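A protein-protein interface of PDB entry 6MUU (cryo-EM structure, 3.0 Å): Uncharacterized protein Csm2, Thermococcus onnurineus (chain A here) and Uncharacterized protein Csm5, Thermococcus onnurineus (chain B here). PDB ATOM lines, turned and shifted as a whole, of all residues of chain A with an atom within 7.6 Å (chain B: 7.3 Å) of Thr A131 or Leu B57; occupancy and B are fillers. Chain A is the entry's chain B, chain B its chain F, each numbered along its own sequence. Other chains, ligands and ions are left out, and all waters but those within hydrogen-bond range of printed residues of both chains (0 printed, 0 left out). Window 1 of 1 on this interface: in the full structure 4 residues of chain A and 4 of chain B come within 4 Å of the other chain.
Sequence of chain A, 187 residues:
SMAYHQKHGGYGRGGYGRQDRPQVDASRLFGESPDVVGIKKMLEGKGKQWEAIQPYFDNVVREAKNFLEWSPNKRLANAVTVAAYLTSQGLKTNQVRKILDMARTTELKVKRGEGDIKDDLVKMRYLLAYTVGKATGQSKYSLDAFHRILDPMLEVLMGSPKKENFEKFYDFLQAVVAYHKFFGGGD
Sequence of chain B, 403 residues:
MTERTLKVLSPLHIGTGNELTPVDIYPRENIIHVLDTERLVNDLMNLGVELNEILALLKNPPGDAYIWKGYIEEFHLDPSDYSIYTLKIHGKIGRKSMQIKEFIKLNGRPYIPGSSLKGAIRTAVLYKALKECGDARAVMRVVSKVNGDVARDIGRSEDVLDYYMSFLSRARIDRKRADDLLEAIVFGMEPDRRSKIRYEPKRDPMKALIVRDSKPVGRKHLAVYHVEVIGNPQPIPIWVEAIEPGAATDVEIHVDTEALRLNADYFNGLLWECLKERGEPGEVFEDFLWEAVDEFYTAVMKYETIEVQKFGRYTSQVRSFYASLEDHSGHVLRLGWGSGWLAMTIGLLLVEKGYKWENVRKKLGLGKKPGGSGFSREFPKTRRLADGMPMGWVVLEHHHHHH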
ATOM      1  N   MET A 124       9.094 -13.845 -26.274  1.00  0.00           N
ATOM      2  CA  MET A 124       8.139 -14.485 -25.378  1.00  0.00           C
ATOM      3  C   MET A 124       6.978 -13.560 -25.051  1.00  0.00           C
ATOM      4  O   MET A 124       5.852 -14.027 -24.843  1.00  0.00           O
ATOM      5  CB  MET A 124       8.838 -14.928 -24.094  1.00  0.00           C
ATOM      6  N   ARG A 125       7.229 -12.250 -25.003  1.00  0.00           N
ATOM      7  CA  ARG A 125       6.154 -11.294 -24.771  1.00  0.00           C
ATOM      8  C   ARG A 125       5.353 -11.025 -26.036  1.00  0.00           C
ATOM      9  O   ARG A 125       4.143 -10.789 -25.955  1.00  0.00           O
ATOM     10  CB  ARG A 125       6.720  -9.985 -24.225  1.00  0.00           C
ATOM     11  N   TYR A 126       6.005 -11.059 -27.204  1.00  0.00           N
ATOM     12  CA  TYR A 126       5.304 -10.821 -28.462  1.00  0.00           C
ATOM     13  C   TYR A 126       4.346 -11.953 -28.795  1.00  0.00           C
ATOM     14  O   TYR A 126       3.370 -11.745 -29.524  1.00  0.00           O
ATOM     15  CB  TYR A 126       6.307 -10.630 -29.597  1.00  0.00           C
ATOM     16  N   LEU A 127       4.606 -13.152 -28.274  1.00  0.00           N
ATOM     17  CA  LEU A 127       3.671 -14.256 -28.434  1.00  0.00           C
ATOM     18  C   LEU A 127       2.518 -14.153 -27.444  1.00  0.00           C
ATOM     19  O   LEU A 127       1.350 -14.260 -27.831  1.00  0.00           O
ATOM     20  CB  LEU A 127       4.403 -15.588 -28.269  1.00  0.00           C
ATOM     21  N   LEU A 128       2.835 -13.931 -26.163  1.00  0.00           N
ATOM     22  CA  LEU A 128       1.822 -13.968 -25.112  1.00  0.00           C
ATOM     23  C   LEU A 128       0.871 -12.782 -25.186  1.00  0.00           C
ATOM     24  O   LEU A 128      -0.290 -12.895 -24.779  1.00  0.00           O
ATOM     25  CB  LEU A 128       2.491 -14.018 -23.738  1.00  0.00           C
ATOM     26  N   ALA A 129       1.339 -11.640 -25.697  1.00  0.00           N
ATOM     27  CA  ALA A 129       0.435 -10.516 -25.908  1.00  0.00           C
ATOM     28  C   ALA A 129      -0.513 -10.779 -27.067  1.00  0.00           C
ATOM     29  O   ALA A 129      -1.639 -10.269 -27.073  1.00  0.00           O
ATOM     30  CB  ALA A 129       1.233  -9.236 -26.147  1.00  0.00           C
ATOM     31  N   TYR A 130      -0.084 -11.581 -28.042  1.00  0.00           N
ATOM     32  CA  TYR A 130      -0.935 -11.971 -29.158  1.00  0.00           C
ATOM     33  C   TYR A 130      -1.943 -13.047 -28.784  1.00  0.00           C
ATOM     34  O   TYR A 130      -2.821 -13.356 -29.598  1.00  0.00           O
ATOM     35  CB  TYR A 130      -0.074 -12.462 -30.324  1.00  0.00           C
ATOM     36  N   THR A 131      -1.835 -13.623 -27.586  1.00  0.00           N
ATOM     37  CA  THR A 131      -2.771 -14.656 -27.160  1.00  0.00           C
ATOM     38  C   THR A 131      -4.144 -14.069 -26.869  1.00  0.00           C
ATOM     39  O   THR A 131      -5.152 -14.506 -27.436  1.00  0.00           O
ATOM     40  CB  THR A 131      -2.227 -15.373 -25.926  1.00  0.00           C
ATOM     41  N   VAL A 132      -4.203 -13.066 -25.993  1.00  0.00           N
ATOM     42  CA  VAL A 132      -5.467 -12.463 -25.574  1.00  0.00           C
ATOM     43  C   VAL A 132      -5.946 -11.435 -26.603  1.00  0.00           C
ATOM     44  O   VAL A 132      -5.975 -10.229 -26.363  1.00  0.00           O
ATOM     45  CB  VAL A 132      -5.314 -11.837 -24.195  1.00  0.00           C
ATOM     46  N   GLY A 133      -6.327 -11.942 -27.775  1.00  0.00           N
ATOM     47  CA  GLY A 133      -6.769 -11.062 -28.850  1.00  0.00           C
ATOM     48  C   GLY A 133      -8.194 -10.578 -28.612  1.00  0.00           C
ATOM     49  O   GLY A 133      -8.438  -9.376 -28.456  1.00  0.00           O
ATOM     50  N   LYS A 134      -9.148 -11.501 -28.573  1.00  0.00           N
ATOM     51  CA  LYS A 134     -10.553 -11.142 -28.427  1.00  0.00           C
ATOM     52  C   LYS A 134     -11.241 -12.038 -27.408  1.00  0.00           C
ATOM     53  O   LYS A 134     -12.299 -12.603 -27.683  1.00  0.00           O
ATOM     54  CB  LYS A 134     -11.261 -11.222 -29.768  1.00  0.00           C
ATOM     55  N   LEU A 143      -4.238  -9.015 -33.906  1.00  0.00           N
ATOM     56  CA  LEU A 143      -2.922  -9.229 -33.322  1.00  0.00           C
ATOM     57  C   LEU A 143      -2.133 -10.297 -34.063  1.00  0.00           C
ATOM     58  O   LEU A 143      -0.899 -10.304 -33.986  1.00  0.00           O
ATOM     59  CB  LEU A 143      -3.049  -9.621 -31.846  1.00  0.00           C
ATOM     60  CG  LEU A 143      -3.212  -8.557 -30.752  1.00  0.00           C
ATOM     61  CD1 LEU A 143      -2.033  -7.590 -30.756  1.00  0.00           C
ATOM     62  CD2 LEU A 143      -4.544  -7.811 -30.816  1.00  0.00           C
ATOM     63  N   HIS A 147       1.575 -10.312 -35.493  1.00  0.00           N
ATOM     64  CA  HIS A 147       2.467 -11.412 -35.152  1.00  0.00           C
ATOM     65  C   HIS A 147       3.115 -12.037 -36.379  1.00  0.00           C
ATOM     66  O   HIS A 147       4.226 -12.568 -36.274  1.00  0.00           O
ATOM     67  CB  HIS A 147       1.706 -12.484 -34.365  1.00  0.00           C
ATOM     68  CG  HIS A 147       2.580 -13.569 -33.820  1.00  0.00           C
ATOM     69  ND1 HIS A 147       2.890 -14.705 -34.535  1.00  0.00           N
ATOM     70  CD2 HIS A 147       3.226 -13.685 -32.636  1.00  0.00           C
ATOM     71  CE1 HIS A 147       3.681 -15.477 -33.812  1.00  0.00           C
ATOM     72  NE2 HIS A 147       3.901 -14.880 -32.656  1.00  0.00           N
ATOM     73  N   THR B  21      -5.532 -14.004 -18.216  1.00  0.00           N
ATOM     74  CA  THR B  21      -5.919 -15.171 -18.978  1.00  0.00           C
ATOM     75  C   THR B  21      -5.406 -16.428 -18.274  1.00  0.00           C
ATOM     76  O   THR B  21      -4.448 -16.363 -17.500  1.00  0.00           O
ATOM     77  CB  THR B  21      -5.360 -15.058 -20.396  1.00  0.00           C
ATOM     78  OG1 THR B  21      -3.932 -15.000 -20.342  1.00  0.00           O
ATOM     79  CG2 THR B  21      -5.876 -13.799 -21.055  1.00  0.00           C
ATOM     80  N   VAL B  23      -3.474 -18.721 -19.008  1.00  0.00           N
ATOM     81  CA  VAL B  23      -2.108 -19.181 -19.234  1.00  0.00           C
ATOM     82  C   VAL B  23      -1.234 -18.860 -18.023  1.00  0.00           C
ATOM     83  O   VAL B  23      -0.275 -19.583 -17.728  1.00  0.00           O
ATOM     84  CB  VAL B  23      -1.553 -18.590 -20.551  1.00  0.00           C
ATOM     85  CG1 VAL B  23      -1.381 -17.081 -20.478  1.00  0.00           C
ATOM     86  CG2 VAL B  23      -0.246 -19.265 -20.957  1.00  0.00           C
ATOM     87  N   LEU B  51       9.986 -23.213 -29.884  1.00  0.00           N
ATOM     88  CA  LEU B  51       8.803 -22.600 -30.478  1.00  0.00           C
ATOM     89  C   LEU B  51       7.520 -23.322 -30.097  1.00  0.00           C
ATOM     90  O   LEU B  51       6.434 -22.772 -30.302  1.00  0.00           O
ATOM     91  CB  LEU B  51       8.936 -22.558 -32.001  1.00  0.00           C
ATOM     92  N   ASN B  52       7.622 -24.538 -29.553  1.00  0.00           N
ATOM     93  CA  ASN B  52       6.440 -25.269 -29.113  1.00  0.00           C
ATOM     94  C   ASN B  52       5.837 -24.678 -27.848  1.00  0.00           C
ATOM     95  O   ASN B  52       4.640 -24.865 -27.602  1.00  0.00           O
ATOM     96  CB  ASN B  52       6.784 -26.740 -28.886  1.00  0.00           C
ATOM     97  N   GLU B  53       6.638 -23.981 -27.038  1.00  0.00           N
ATOM     98  CA  GLU B  53       6.093 -23.284 -25.879  1.00  0.00           C
ATOM     99  C   GLU B  53       5.239 -22.098 -26.308  1.00  0.00           C
ATOM    100  O   GLU B  53       4.171 -21.854 -25.737  1.00  0.00           O
ATOM    101  CB  GLU B  53       7.223 -22.825 -24.959  1.00  0.00           C
ATOM    102  N   ILE B  54       5.690 -21.360 -27.322  1.00  0.00           N
ATOM    103  CA  ILE B  54       4.943 -20.201 -27.793  1.00  0.00           C
ATOM    104  C   ILE B  54       3.763 -20.594 -28.666  1.00  0.00           C
ATOM    105  O   ILE B  54       2.783 -19.847 -28.741  1.00  0.00           O
ATOM    106  CB  ILE B  54       5.865 -19.256 -28.564  1.00  0.00           C
ATOM    107  N   LEU B  55       3.842 -21.749 -29.334  1.00  0.00           N
ATOM    108  CA  LEU B  55       2.753 -22.181 -30.204  1.00  0.00           C
ATOM    109  C   LEU B  55       1.511 -22.553 -29.407  1.00  0.00           C
ATOM    110  O   LEU B  55       0.389 -22.291 -29.853  1.00  0.00           O
ATOM    111  CB  LEU B  55       3.206 -23.359 -31.065  1.00  0.00           C
ATOM    112  N   ALA B  56       1.691 -23.156 -28.231  1.00  0.00           N
ATOM    113  CA  ALA B  56       0.562 -23.367 -27.334  1.00  0.00           C
ATOM    114  C   ALA B  56       0.127 -22.064 -26.682  1.00  0.00           C
ATOM    115  O   ALA B  56      -1.047 -21.908 -26.330  1.00  0.00           O
ATOM    116  CB  ALA B  56       0.920 -24.402 -26.269  1.00  0.00           C
ATOM    117  N   LEU B  57       1.055 -21.119 -26.517  1.00  0.00           N
ATOM    118  CA  LEU B  57       0.702 -19.827 -25.943  1.00  0.00           C
ATOM    119  C   LEU B  57      -0.074 -18.977 -26.940  1.00  0.00           C
ATOM    120  O   LEU B  57      -1.106 -18.394 -26.594  1.00  0.00           O
ATOM    121  CB  LEU B  57       1.960 -19.097 -25.474  1.00  0.00           C
ATOM    122  N   LEU B  58       0.393 -18.915 -28.190  1.00  0.00           N
ATOM    123  CA  LEU B  58      -0.290 -18.144 -29.221  1.00  0.00           C
ATOM    124  C   LEU B  58      -1.589 -18.787 -29.687  1.00  0.00           C
ATOM    125  O   LEU B  58      -2.386 -18.116 -30.350  1.00  0.00           O
ATOM    126  CB  LEU B  58       0.636 -17.935 -30.422  1.00  0.00           C
ATOM    127  N   LYS B  59      -1.818 -20.062 -29.368  1.00  0.00           N
ATOM    128  CA  LYS B  59      -3.062 -20.714 -29.762  1.00  0.00           C
ATOM    129  C   LYS B  59      -4.232 -20.219 -28.924  1.00  0.00           C
ATOM    130  O   LYS B  59      -5.262 -19.804 -29.471  1.00  0.00           O
ATOM    131  CB  LYS B  59      -2.922 -22.231 -29.641  1.00  0.00           C
ATOM    132  N   ASN B  60      -4.067 -20.239 -27.593  1.00  0.00           N
ATOM    133  CA  ASN B  60      -5.117 -19.967 -26.601  1.00  0.00           C
ATOM    134  C   ASN B  60      -6.358 -20.821 -26.857  1.00  0.00           C
ATOM    135  O   ASN B  60      -7.494 -20.340 -26.855  1.00  0.00           O
ATOM    136  CB  ASN B  60      -5.466 -18.476 -26.544  1.00  0.00           C
ATOM    137  N   PRO B  61      -6.125 -22.107 -27.089  1.00  0.00           N
ATOM    138  CA  PRO B  61      -7.172 -23.062 -27.415  1.00  0.00           C
ATOM    139  C   PRO B  61      -7.348 -24.043 -26.260  1.00  0.00           C
ATOM    140  O   PRO B  61      -6.630 -23.982 -25.257  1.00  0.00           O
ATOM    141  CB  PRO B  61      -6.852 -23.798 -28.720  1.00  0.00           C
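Printed residues of chain B within 4 Å of Leu A127: Ile B54.
Thr A131 touches just one residue of chain B: Leu B57.
Of the printed residues of chain B, Val A132 touches Thr B21 (3.7 Å).
No residue of chain A comes within 4 Å of Ala B56.
Of chain A, only Thr A131 comes within 4 Å of Leu B57.
The nearest residue of chain B that does not touch Thr A131 is Asn B60 (4.1 Å).
The nearest residue of chain A that does not touch Leu B57 is Leu A127 (5.0 Å).
The nearest printed residue of chain A that does not touch Thr B21 is Thr A131 (5.9 Å).
Among the printed residues, pairs that only touch across the chains: Thr A131 with Leu B57, Val A132 with Thr B21 and Leu A127 with Ile B54.
Of the 13 printed residues of chain B, 3 touch a printed residue of chain A.
Printed residues of chain B that touch a printed residue of chain A: Thr B21, Ile B54 and Leu B57.
Hydrophobic or aromatic side chains of chain B within 4 Å of the printed part of chain A: Ile B54.
Of the 13 printed residues of chain A, 3 touch a printed residue of chain B.
Printed residues of chain A that touch a printed residue of chain B: Leu A127, Thr A131 and Val A132.
Hydrophobic or aromatic side chains of chain A within 4 Å of the printed part of chain B: Leu A127 and Val A132.
Along chain A the printed residues that touch a printed residue of chain B span positions 127 to 132.
Among the printed residues, 3 pairs touch across the chains.
Among the printed residues, no Asp or Glu carboxylate lies within 4 Å of a Lys or Arg side-chain nitrogen of the other chain.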
